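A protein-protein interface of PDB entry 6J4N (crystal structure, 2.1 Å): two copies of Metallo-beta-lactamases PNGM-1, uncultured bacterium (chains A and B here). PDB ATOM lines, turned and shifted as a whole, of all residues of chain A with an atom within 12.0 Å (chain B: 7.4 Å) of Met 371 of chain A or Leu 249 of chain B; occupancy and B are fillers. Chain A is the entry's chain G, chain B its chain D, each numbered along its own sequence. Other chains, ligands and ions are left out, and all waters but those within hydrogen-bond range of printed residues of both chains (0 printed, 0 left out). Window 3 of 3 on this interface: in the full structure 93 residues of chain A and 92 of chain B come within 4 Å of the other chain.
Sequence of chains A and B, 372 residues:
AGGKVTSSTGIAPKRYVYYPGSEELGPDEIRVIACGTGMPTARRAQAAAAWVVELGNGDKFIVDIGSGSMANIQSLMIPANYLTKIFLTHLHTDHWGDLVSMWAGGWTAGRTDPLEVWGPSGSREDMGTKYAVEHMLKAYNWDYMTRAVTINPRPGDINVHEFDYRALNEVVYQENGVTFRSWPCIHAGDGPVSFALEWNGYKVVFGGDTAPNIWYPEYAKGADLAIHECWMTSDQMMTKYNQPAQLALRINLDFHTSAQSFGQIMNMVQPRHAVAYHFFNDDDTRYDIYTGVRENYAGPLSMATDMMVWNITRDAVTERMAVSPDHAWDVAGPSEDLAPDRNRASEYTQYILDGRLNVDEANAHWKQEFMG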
ATOM      1  N   ARG A 356     -20.531  15.794 -10.266  1.00  0.00           N
ATOM      2  CA  ARG A 356     -20.867  14.349 -10.303  1.00  0.00           C
ATOM      3  C   ARG A 356     -20.907  13.905 -11.767  1.00  0.00           C
ATOM      4  O   ARG A 356     -21.541  14.555 -12.530  1.00  0.00           O
ATOM      5  CB  ARG A 356     -22.227  14.007  -9.683  1.00  0.00           C
ATOM      6  CG  ARG A 356     -22.255  13.943  -8.170  1.00  0.00           C
ATOM      7  CD  ARG A 356     -23.229  12.909  -7.661  1.00  0.00           C
ATOM      8  NE  ARG A 356     -23.412  13.137  -6.230  1.00  0.00           N
ATOM      9  CZ  ARG A 356     -22.752  12.544  -5.225  1.00  0.00           C
ATOM     10  NH1 ARG A 356     -21.839  11.612  -5.443  1.00  0.00           N
ATOM     11  NH2 ARG A 356     -23.051  12.867  -3.977  1.00  0.00           N
ATOM     12  N   VAL A 359     -22.914   8.000 -14.791  1.00  0.00           N
ATOM     13  CA  VAL A 359     -22.416   6.595 -14.932  1.00  0.00           C
ATOM     14  C   VAL A 359     -23.605   5.629 -15.121  1.00  0.00           C
ATOM     15  O   VAL A 359     -23.418   4.424 -14.903  1.00  0.00           O
ATOM     16  CB  VAL A 359     -21.542   6.214 -13.710  1.00  0.00           C
ATOM     17  CG1 VAL A 359     -20.238   7.000 -13.701  1.00  0.00           C
ATOM     18  CG2 VAL A 359     -22.255   6.419 -12.372  1.00  0.00           C
ATOM     19  N   ASP A 360     -24.794   6.126 -15.492  1.00  0.00           N
ATOM     20  CA  ASP A 360     -26.045   5.305 -15.565  1.00  0.00           C
ATOM     21  C   ASP A 360     -25.880   4.103 -16.511  1.00  0.00           C
ATOM     22  O   ASP A 360     -26.119   2.951 -16.096  1.00  0.00           O
ATOM     23  CB  ASP A 360     -27.226   6.150 -16.053  1.00  0.00           C
ATOM     24  CG  ASP A 360     -27.734   7.166 -15.045  1.00  0.00           C
ATOM     25  OD1 ASP A 360     -27.473   6.987 -13.837  1.00  0.00           O
ATOM     26  OD2 ASP A 360     -28.396   8.127 -15.480  1.00  0.00           O
ATOM     27  N   ALA A 362     -23.077   2.855 -17.785  1.00  0.00           N
ATOM     28  CA  ALA A 362     -21.963   1.973 -17.349  1.00  0.00           C
ATOM     29  C   ALA A 362     -22.448   0.940 -16.315  1.00  0.00           C
ATOM     30  O   ALA A 362     -21.898  -0.168 -16.281  1.00  0.00           O
ATOM     31  CB  ALA A 362     -20.825   2.816 -16.818  1.00  0.00           C
ATOM     32  N   ASN A 363     -23.447   1.291 -15.504  1.00  0.00           N
ATOM     33  CA  ASN A 363     -23.864   0.516 -14.305  1.00  0.00           C
ATOM     34  C   ASN A 363     -25.224  -0.183 -14.484  1.00  0.00           C
ATOM     35  O   ASN A 363     -25.628  -0.930 -13.551  1.00  0.00           O
ATOM     36  CB  ASN A 363     -23.968   1.444 -13.103  1.00  0.00           C
ATOM     37  CG  ASN A 363     -22.611   1.791 -12.541  1.00  0.00           C
ATOM     38  OD1 ASN A 363     -22.185   1.189 -11.550  1.00  0.00           O
ATOM     39  ND2 ASN A 363     -21.925   2.739 -13.170  1.00  0.00           N
ATOM     40  N   ALA A 364     -25.918   0.058 -15.601  1.00  0.00           N
ATOM     41  CA  ALA A 364     -27.316  -0.391 -15.800  1.00  0.00           C
ATOM     42  C   ALA A 364     -27.349  -1.922 -15.758  1.00  0.00           C
ATOM     43  O   ALA A 364     -28.239  -2.507 -15.077  1.00  0.00           O
ATOM     44  CB  ALA A 364     -27.874   0.148 -17.098  1.00  0.00           C
ATOM     45  N   HIS A 365     -26.376  -2.550 -16.416  1.00  0.00           N
ATOM     46  CA  HIS A 365     -26.316  -4.030 -16.550  1.00  0.00           C
ATOM     47  C   HIS A 365     -26.355  -4.692 -15.161  1.00  0.00           C
ATOM     48  O   HIS A 365     -27.303  -5.492 -14.918  1.00  0.00           O
ATOM     49  CB  HIS A 365     -25.114  -4.471 -17.395  1.00  0.00           C
ATOM     50  CG  HIS A 365     -25.411  -5.679 -18.220  1.00  0.00           C
ATOM     51  ND1 HIS A 365     -25.995  -6.820 -17.681  1.00  0.00           N
ATOM     52  CD2 HIS A 365     -25.226  -5.932 -19.536  1.00  0.00           C
ATOM     53  CE1 HIS A 365     -26.150  -7.723 -18.629  1.00  0.00           C
ATOM     54  NE2 HIS A 365     -25.682  -7.204 -19.775  1.00  0.00           N
ATOM     55  N   TRP A 366     -25.407  -4.378 -14.270  1.00  0.00           N
ATOM     56  CA  TRP A 366     -25.315  -5.040 -12.934  1.00  0.00           C
ATOM     57  C   TRP A 366     -26.475  -4.584 -12.032  1.00  0.00           C
ATOM     58  O   TRP A 366     -26.947  -5.430 -11.247  1.00  0.00           O
ATOM     59  CB  TRP A 366     -23.941  -4.860 -12.251  1.00  0.00           C
ATOM     60  CG  TRP A 366     -23.743  -3.537 -11.581  1.00  0.00           C
ATOM     61  CD1 TRP A 366     -23.141  -2.433 -12.117  1.00  0.00           C
ATOM     62  CD2 TRP A 366     -24.159  -3.160 -10.253  1.00  0.00           C
ATOM     63  NE1 TRP A 366     -23.162  -1.401 -11.216  1.00  0.00           N
ATOM     64  CE2 TRP A 366     -23.780  -1.813 -10.068  1.00  0.00           C
ATOM     65  CE3 TRP A 366     -24.826  -3.815  -9.212  1.00  0.00           C
ATOM     66  CZ2 TRP A 366     -24.042  -1.115  -8.888  1.00  0.00           C
ATOM     67  CZ3 TRP A 366     -25.097  -3.121  -8.051  1.00  0.00           C
ATOM     68  CH2 TRP A 366     -24.698  -1.793  -7.886  1.00  0.00           C
ATOM     69  N   LYS A 367     -26.903  -3.315 -12.101  1.00  0.00           N
ATOM     70  CA  LYS A 367     -28.040  -2.800 -11.275  1.00  0.00           C
ATOM     71  C   LYS A 367     -29.292  -3.665 -11.502  1.00  0.00           C
ATOM     72  O   LYS A 367     -29.925  -4.104 -10.504  1.00  0.00           O
ATOM     73  CB  LYS A 367     -28.369  -1.339 -11.612  1.00  0.00           C
ATOM     74  CG  LYS A 367     -27.944  -0.311 -10.571  1.00  0.00           C
ATOM     75  CD  LYS A 367     -27.258   0.905 -11.181  1.00  0.00           C
ATOM     76  CE  LYS A 367     -28.201   1.867 -11.875  1.00  0.00           C
ATOM     77  NZ  LYS A 367     -29.150   2.481 -10.915  1.00  0.00           N
ATOM     78  N   GLN A 368     -29.617  -3.896 -12.775  1.00  0.00           N
ATOM     79  CA  GLN A 368     -30.843  -4.596 -13.248  1.00  0.00           C
ATOM     80  C   GLN A 368     -30.799  -6.057 -12.772  1.00  0.00           C
ATOM     81  O   GLN A 368     -31.821  -6.522 -12.213  1.00  0.00           O
ATOM     82  CB  GLN A 368     -30.920  -4.402 -14.767  1.00  0.00           C
ATOM     83  CG  GLN A 368     -31.868  -5.319 -15.529  1.00  0.00           C
ATOM     84  CD  GLN A 368     -32.006  -4.844 -16.961  1.00  0.00           C
ATOM     85  OE1 GLN A 368     -33.079  -4.889 -17.556  1.00  0.00           O
ATOM     86  NE2 GLN A 368     -30.919  -4.340 -17.525  1.00  0.00           N
ATOM     87  N   GLU A 369     -29.671  -6.758 -12.963  1.00  0.00           N
ATOM     88  CA  GLU A 369     -29.473  -8.132 -12.409  1.00  0.00           C
ATOM     89  C   GLU A 369     -29.597  -8.093 -10.870  1.00  0.00           C
ATOM     90  O   GLU A 369     -30.288  -8.977 -10.345  1.00  0.00           O
ATOM     91  CB  GLU A 369     -28.157  -8.742 -12.911  1.00  0.00           C
ATOM     92  CG  GLU A 369     -28.017 -10.255 -12.716  1.00  0.00           C
ATOM     93  CD  GLU A 369     -27.615 -10.704 -11.314  1.00  0.00           C
ATOM     94  OE1 GLU A 369     -27.039  -9.877 -10.570  1.00  0.00           O
ATOM     95  OE2 GLU A 369     -27.884 -11.877 -10.952  1.00  0.00           O
ATOM     96  N   PHE A 370     -29.018  -7.101 -10.166  1.00  0.00           N
ATOM     97  CA  PHE A 370     -28.972  -7.045  -8.670  1.00  0.00           C
ATOM     98  C   PHE A 370     -30.352  -6.723  -8.091  1.00  0.00           C
ATOM     99  O   PHE A 370     -30.692  -7.223  -6.986  1.00  0.00           O
ATOM    100  CB  PHE A 370     -27.966  -6.016  -8.131  1.00  0.00           C
ATOM    101  CG  PHE A 370     -27.925  -5.874  -6.619  1.00  0.00           C
ATOM    102  CD1 PHE A 370     -27.240  -6.795  -5.826  1.00  0.00           C
ATOM    103  CD2 PHE A 370     -28.556  -4.811  -5.976  1.00  0.00           C
ATOM    104  CE1 PHE A 370     -27.190  -6.661  -4.443  1.00  0.00           C
ATOM    105  CE2 PHE A 370     -28.516  -4.687  -4.594  1.00  0.00           C
ATOM    106  CZ  PHE A 370     -27.829  -5.607  -3.830  1.00  0.00           C
ATOM    107  N   MET A 371     -31.116  -5.886  -8.784  1.00  0.00           N
ATOM    108  CA  MET A 371     -32.473  -5.487  -8.327  1.00  0.00           C
ATOM    109  C   MET A 371     -33.468  -6.624  -8.620  1.00  0.00           C
ATOM    110  O   MET A 371     -34.328  -6.870  -7.755  1.00  0.00           O
ATOM    111  CB  MET A 371     -32.865  -4.153  -8.969  1.00  0.00           C
ATOM    112  CG  MET A 371     -31.939  -3.027  -8.516  1.00  0.00           C
ATOM    113  SD  MET A 371     -32.257  -1.402  -9.234  1.00  0.00           S
ATOM    114  CE  MET A 371     -32.987  -0.608  -7.801  1.00  0.00           C
ATOM    115  N   GLY A 372     -33.305  -7.339  -9.742  1.00  0.00           N
ATOM    116  CA  GLY A 372     -34.101  -8.536 -10.107  1.00  0.00           C
ATOM    117  C   GLY A 372     -34.510  -9.381  -8.904  1.00  0.00           C
ATOM    118  O   GLY A 372     -33.678 -10.016  -8.252  1.00  0.00           O
ATOM    119  N   SER B 234     -21.824  -4.776  -4.514  1.00  0.00           N
ATOM    120  CA  SER B 234     -23.010  -4.636  -3.638  1.00  0.00           C
ATOM    121  C   SER B 234     -23.323  -6.017  -3.056  1.00  0.00           C
ATOM    122  O   SER B 234     -23.715  -6.077  -1.883  1.00  0.00           O
ATOM    123  CB  SER B 234     -24.191  -4.046  -4.366  1.00  0.00           C
ATOM    124  OG  SER B 234     -23.934  -2.713  -4.785  1.00  0.00           O
ATOM    125  N   ASP B 235     -23.102  -7.097  -3.805  1.00  0.00           N
ATOM    126  CA  ASP B 235     -23.323  -8.468  -3.257  1.00  0.00           C
ATOM    127  C   ASP B 235     -22.376  -8.676  -2.068  1.00  0.00           C
ATOM    128  O   ASP B 235     -22.824  -9.213  -1.022  1.00  0.00           O
ATOM    129  CB  ASP B 235     -23.176  -9.560  -4.318  1.00  0.00           C
ATOM    130  CG  ASP B 235     -24.353  -9.587  -5.289  1.00  0.00           C
ATOM    131  OD1 ASP B 235     -24.128  -9.840  -6.497  1.00  0.00           O
ATOM    132  OD2 ASP B 235     -25.495  -9.334  -4.830  1.00  0.00           O
ATOM    133  N   MET B 237     -21.156  -6.298  -0.140  1.00  0.00           N
ATOM    134  CA  MET B 237     -21.705  -5.397   0.908  1.00  0.00           C
ATOM    135  C   MET B 237     -22.790  -6.147   1.709  1.00  0.00           C
ATOM    136  O   MET B 237     -22.835  -5.960   2.964  1.00  0.00           O
ATOM    137  CB  MET B 237     -22.285  -4.127   0.275  1.00  0.00           C
ATOM    138  CG  MET B 237     -21.245  -3.153  -0.355  1.00  0.00           C
ATOM    139  SD  MET B 237     -19.729  -2.833   0.627  1.00  0.00           S
ATOM    140  CE  MET B 237     -20.416  -2.260   2.179  1.00  0.00           C
ATOM    141  N   MET B 238     -23.583  -7.010   1.045  1.00  0.00           N
ATOM    142  CA  MET B 238     -24.573  -7.911   1.713  1.00  0.00           C
ATOM    143  C   MET B 238     -23.878  -9.104   2.405  1.00  0.00           C
ATOM    144  O   MET B 238     -24.041  -9.225   3.609  1.00  0.00           O
ATOM    145  CB  MET B 238     -25.637  -8.390   0.724  1.00  0.00           C
ATOM    146  CG  MET B 238     -26.496  -7.228   0.226  1.00  0.00           C
ATOM    147  SD  MET B 238     -27.861  -7.744  -0.856  1.00  0.00           S
ATOM    148  CE  MET B 238     -28.896  -8.649   0.303  1.00  0.00           C
ATOM    149  N   GLN B 243     -25.362  -5.885   4.811  1.00  0.00           N
ATOM    150  CA  GLN B 243     -26.157  -4.673   4.455  1.00  0.00           C
ATOM    151  C   GLN B 243     -27.490  -5.106   3.843  1.00  0.00           C
ATOM    152  O   GLN B 243     -27.539  -6.134   3.165  1.00  0.00           O
ATOM    153  CB  GLN B 243     -25.421  -3.768   3.454  1.00  0.00           C
ATOM    154  CG  GLN B 243     -24.254  -2.955   4.020  1.00  0.00           C
ATOM    155  CD  GLN B 243     -24.552  -2.273   5.335  1.00  0.00           C
ATOM    156  OE1 GLN B 243     -25.319  -1.310   5.410  1.00  0.00           O
ATOM    157  NE2 GLN B 243     -23.931  -2.769   6.395  1.00  0.00           N
ATOM    158  N   PRO B 244     -28.606  -4.349   4.048  1.00  0.00           N
ATOM    159  CA  PRO B 244     -29.833  -4.584   3.281  1.00  0.00           C
ATOM    160  C   PRO B 244     -29.577  -4.262   1.798  1.00  0.00           C
ATOM    161  O   PRO B 244     -28.711  -3.437   1.526  1.00  0.00           O
ATOM    162  CB  PRO B 244     -30.882  -3.639   3.901  1.00  0.00           C
ATOM    163  CG  PRO B 244     -30.275  -3.171   5.219  1.00  0.00           C
ATOM    164  CD  PRO B 244     -28.770  -3.246   5.019  1.00  0.00           C
ATOM    165  N   ALA B 245     -30.310  -4.918   0.891  1.00  0.00           N
ATOM    166  CA  ALA B 245     -30.170  -4.804  -0.585  1.00  0.00           C
ATOM    167  C   ALA B 245     -30.151  -3.331  -1.053  1.00  0.00           C
ATOM    168  O   ALA B 245     -29.320  -2.974  -1.931  1.00  0.00           O
ATOM    169  CB  ALA B 245     -31.283  -5.587  -1.244  1.00  0.00           C
ATOM    170  N   GLN B 246     -31.026  -2.501  -0.482  1.00  0.00           N
ATOM    171  CA  GLN B 246     -31.239  -1.074  -0.877  1.00  0.00           C
ATOM    172  C   GLN B 246     -29.962  -0.249  -0.614  1.00  0.00           C
ATOM    173  O   GLN B 246     -29.417   0.347  -1.570  1.00  0.00           O
ATOM    174  CB  GLN B 246     -32.486  -0.550  -0.144  1.00  0.00           C
ATOM    175  CG  GLN B 246     -32.610   0.971  -0.023  1.00  0.00           C
ATOM    176  CD  GLN B 246     -32.551   1.728  -1.331  1.00  0.00           C
ATOM    177  OE1 GLN B 246     -32.943   1.230  -2.387  1.00  0.00           O
ATOM    178  NE2 GLN B 246     -32.047   2.954  -1.268  1.00  0.00           N
ATOM    179  N   LEU B 247     -29.517  -0.180   0.642  1.00  0.00           N
ATOM    180  CA  LEU B 247     -28.278   0.561   1.017  1.00  0.00           C
ATOM    181  C   LEU B 247     -27.049  -0.135   0.386  1.00  0.00           C
ATOM    182  O   LEU B 247     -26.067   0.573   0.122  1.00  0.00           O
ATOM    183  CB  LEU B 247     -28.146   0.652   2.547  1.00  0.00           C
ATOM    184  CG  LEU B 247     -28.713   1.864   3.318  1.00  0.00           C
ATOM    185  CD1 LEU B 247     -29.867   2.613   2.640  1.00  0.00           C
ATOM    186  CD2 LEU B 247     -29.132   1.413   4.717  1.00  0.00           C
ATOM    187  N   ALA B 248     -27.079  -1.454   0.141  1.00  0.00           N
ATOM    188  CA  ALA B 248     -25.972  -2.172  -0.539  1.00  0.00           C
ATOM    189  C   ALA B 248     -25.810  -1.594  -1.950  1.00  0.00           C
ATOM    190  O   ALA B 248     -24.655  -1.363  -2.394  1.00  0.00           O
ATOM    191  CB  ALA B 248     -26.211  -3.663  -0.583  1.00  0.00           C
ATOM    192  N   LEU B 249     -26.939  -1.349  -2.618  1.00  0.00           N
ATOM    193  CA  LEU B 249     -26.968  -0.819  -4.008  1.00  0.00           C
ATOM    194  C   LEU B 249     -26.424   0.611  -4.009  1.00  0.00           C
ATOM    195  O   LEU B 249     -25.544   0.898  -4.849  1.00  0.00           O
ATOM    196  CB  LEU B 249     -28.411  -0.874  -4.520  1.00  0.00           C
ATOM    197  CG  LEU B 249     -28.758  -0.087  -5.788  1.00  0.00           C
ATOM    198  CD1 LEU B 249     -28.079  -0.657  -7.038  1.00  0.00           C
ATOM    199  CD2 LEU B 249     -30.278  -0.080  -5.944  1.00  0.00           C
ATOM    200  N   ARG B 250     -26.925   1.465  -3.105  1.00  0.00           N
ATOM    201  CA  ARG B 250     -26.629   2.930  -3.102  1.00  0.00           C
ATOM    202  C   ARG B 250     -25.140   3.175  -2.830  1.00  0.00           C
ATOM    203  O   ARG B 250     -24.616   4.235  -3.253  1.00  0.00           O
ATOM    204  CB  ARG B 250     -27.460   3.689  -2.055  1.00  0.00           C
ATOM    205  CG  ARG B 250     -28.941   3.854  -2.377  1.00  0.00           C
ATOM    206  CD  ARG B 250     -29.208   4.837  -3.507  1.00  0.00           C
ATOM    207  NE  ARG B 250     -29.069   4.224  -4.825  1.00  0.00           N
ATOM    208  CZ  ARG B 250     -28.976   4.880  -5.986  1.00  0.00           C
ATOM    209  NH1 ARG B 250     -28.988   6.201  -6.034  1.00  0.00           N
ATOM    210  NH2 ARG B 250     -28.855   4.197  -7.110  1.00  0.00           N
ATOM    211  N   ILE B 251     -24.482   2.252  -2.126  1.00  0.00           N
ATOM    212  CA  ILE B 251     -23.034   2.393  -1.804  1.00  0.00           C
ATOM    213  C   ILE B 251     -22.249   2.507  -3.116  1.00  0.00           C
ATOM    214  O   ILE B 251     -21.437   3.463  -3.262  1.00  0.00           O
ATOM    215  CB  ILE B 251     -22.564   1.227  -0.919  1.00  0.00           C
ATOM    216  CG1 ILE B 251     -23.007   1.462   0.529  1.00  0.00           C
ATOM    217  CG2 ILE B 251     -21.056   1.012  -1.052  1.00  0.00           C
ATOM    218  CD1 ILE B 251     -23.150   0.197   1.354  1.00  0.00           C
ATOM    219  N   ASN B 252     -22.509   1.587  -4.045  1.00  0.00           N
ATOM    220  CA  ASN B 252     -21.767   1.498  -5.333  1.00  0.00           C
ATOM    221  C   ASN B 252     -22.223   2.577  -6.321  1.00  0.00           C
ATOM    222  O   ASN B 252     -21.634   2.622  -7.415  1.00  0.00           O
ATOM    223  CB  ASN B 252     -21.901   0.105  -5.946  1.00  0.00           C
ATOM    224  CG  ASN B 252     -20.793  -0.837  -5.517  1.00  0.00           C
ATOM    225  OD1 ASN B 252     -19.722  -0.795  -6.095  1.00  0.00           O
ATOM    226  ND2 ASN B 252     -21.029  -1.687  -4.527  1.00  0.00           N
ATOM    227  N   LEU B 253     -23.240   3.391  -5.989  1.00  0.00           N
ATOM    228  CA  LEU B 253     -23.747   4.448  -6.916  1.00  0.00           C
ATOM    229  C   LEU B 253     -23.495   5.844  -6.352  1.00  0.00           C
ATOM    230  O   LEU B 253     -22.947   6.694  -7.081  1.00  0.00           O
ATOM    231  CB  LEU B 253     -25.240   4.250  -7.198  1.00  0.00           C
ATOM    232  CG  LEU B 253     -25.605   3.281  -8.325  1.00  0.00           C
ATOM    233  CD1 LEU B 253     -24.536   3.210  -9.408  1.00  0.00           C
ATOM    234  CD2 LEU B 253     -25.908   1.897  -7.768  1.00  0.00           C
ATOM    235  N   ASP B 254     -23.895   6.090  -5.115  1.00  0.00           N
ATOM    236  CA  ASP B 254     -23.831   7.466  -4.586  1.00  0.00           C
ATOM    237  C   ASP B 254     -22.491   7.691  -3.894  1.00  0.00           C
ATOM    238  O   ASP B 254     -21.871   8.729  -4.145  1.00  0.00           O
ATOM    239  CB  ASP B 254     -25.011   7.729  -3.664  1.00  0.00           C
ATOM    240  CG  ASP B 254     -26.349   7.491  -4.339  1.00  0.00           C
ATOM    241  OD1 ASP B 254     -26.368   7.294  -5.585  1.00  0.00           O
ATOM    242  OD2 ASP B 254     -27.358   7.470  -3.609  1.00  0.00           O
ATOM    243  N   PHE B 255     -22.064   6.766  -3.047  1.00  0.00           N
ATOM    244  CA  PHE B 255     -20.968   7.043  -2.087  1.00  0.00           C
ATOM    245  C   PHE B 255     -19.616   6.727  -2.728  1.00  0.00           C
ATOM    246  O   PHE B 255     -18.619   7.405  -2.463  1.00  0.00           O
ATOM    247  CB  PHE B 255     -21.237   6.315  -0.769  1.00  0.00           C
ATOM    248  CG  PHE B 255     -22.528   6.736  -0.101  1.00  0.00           C
ATOM    249  CD1 PHE B 255     -22.611   7.933   0.606  1.00  0.00           C
ATOM    250  CD2 PHE B 255     -23.680   5.965  -0.216  1.00  0.00           C
ATOM    251  CE1 PHE B 255     -23.799   8.328   1.208  1.00  0.00           C
ATOM    252  CE2 PHE B 255     -24.872   6.364   0.380  1.00  0.00           C
ATOM    253  CZ  PHE B 255     -24.931   7.547   1.091  1.00  0.00           C
ATOM    254  N   SER B 258     -18.051   2.389  -8.241  1.00  0.00           N
ATOM    255  CA  SER B 258     -18.202   0.935  -8.540  1.00  0.00           C
ATOM    256  C   SER B 258     -17.154   0.456  -9.550  1.00  0.00           C
ATOM    257  O   SER B 258     -16.623   1.280 -10.289  1.00  0.00           O
ATOM    258  CB  SER B 258     -19.556   0.663  -9.139  1.00  0.00           C
ATOM    259  OG  SER B 258     -19.540   1.185 -10.460  1.00  0.00           O
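Among the printed residues, merely in contact across the chains: Phe 370 of chain A with Asp 235 of chain B (3.2 Å), Phe 370 of chain A with Ala 245 of chain B (3.3 Å), Trp 366 of chain A with Ser 234 of chain B (3.3 Å), Met 371 of chain A with Leu 249 of chain B (3.3 Å), Lys 367 of chain A with Leu 249 of chain B (3.6 Å), Phe 370 of chain A with Met 238 of chain B (3.7 Å), Trp 366 of chain A with Leu 249 of chain B (3.7 Å), Trp 366 of chain A with Leu 253 of chain B (3.7 Å), Asn 363 of chain A with Leu 253 of chain B (3.8 Å), Lys 367 of chain A with Leu 253 of chain B (3.8 Å), Phe 370 of chain A with Leu 249 of chain B (3.8 Å), Trp 366 of chain A with Asn 252 of chain B (3.8 Å) and Phe 370 of chain A with Ser 234 of chain B (3.98 Å).
No position is printed for both chains.
Of the 15 pairs that touch across the chains among the printed residues, none has its exchanged pair printed and touching as well.
The side-chain hydroxyl of Ser 234 of chain B sits at hydrogen-bond distance from the backbone carbonyl oxygen of Ala 248 of chain B, at 2.8 Å.
The side-chain amide oxygen (OD1) of Asn 363 of chain A sits at hydrogen-bond distance from the indole nitrogen (NE1) of Trp 366 of chain A (2.8 Å).
NH1 of Arg 250 of chain B is in salt-bridge range of OD1 of Asp 254 of chain B (2.9 Å).
The backbone carbonyl oxygen (O) of Val 359 of chain A is in hydrogen-bond range of the side-chain amide nitrogen (ND2) of Asn 363 of chain A.
ND2 of Asn 252 of chain B lies within hydrogen-bond range of OG of Ser 234 of chain B.
Printed residues of chain B that touch a printed residue of chain A: Ser 234, Asp 235, Met 238, Ala 245, Leu 249, Asn 252, Leu 253, Asp 254 and Ser 258.
Hydrophobic or aromatic side chains of chain B within 4 Å of the printed part of chain A: Met 238, Leu 249 and Leu 253.
Of the 14 printed residues of chain A, 6 touch a printed residue of chain B.
Printed residues of chain A that touch a printed residue of chain B: Arg 356, Asn 363, Trp 366, Lys 367, Phe 370 and Met 371.
Among the printed residues, no Asp or Glu carboxylate lies within 4 Å of a Lys or Arg side-chain nitrogen of the other chain.
NH1 of Arg 356 of chain A sits at hydrogen-bond distance from O of Asp 254 of chain B.
The side-chain hydroxyl (OG) of Ser 258 of chain B is in hydrogen-bond range of the side-chain amide oxygen (OD1) of Asn 363 of chain A (2.9 Å).
Met 371 of chain A touches just one residue of chain B: Leu 249 (3.3 Å).
Leu 249 of chain B touches just these residues of chain A: Trp 366, Lys 367, Phe 370 and Met 371.
No residue of chain B comes within 4 Å of Gly 372 of chain A.
Leu 253 of chain B touches just these residues of chain A: Asn 363 (3.8 Å), Trp 366 (3.7 Å) and Lys 367 (3.8 Å).
Printed residues of chain B within 4 Å of Arg 356 of chain A: Asp 254.
Printed residues of chain A within 4 Å of Ser 258 of chain B: Asn 363 (2.9 Å).
Of the printed residues of chain A, Met 238 of chain B touches Phe 370.
Printed residues of chain B within 4 Å of Asn 363 of chain A: Leu 253 and Ser 258.
Of the printed residues of chain A, Asp 254 of chain B touches Arg 356 (3.2 Å).
Leu 247 of chain B touches none of the printed residues of chain A.
The nearest residue of chain B that does not touch Met 371 of chain A is Gln 246 of chain B (5.7 Å).
The nearest printed residue of chain A that does not touch Asp 254 of chain B is Val 359 of chain A (7.4 Å).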
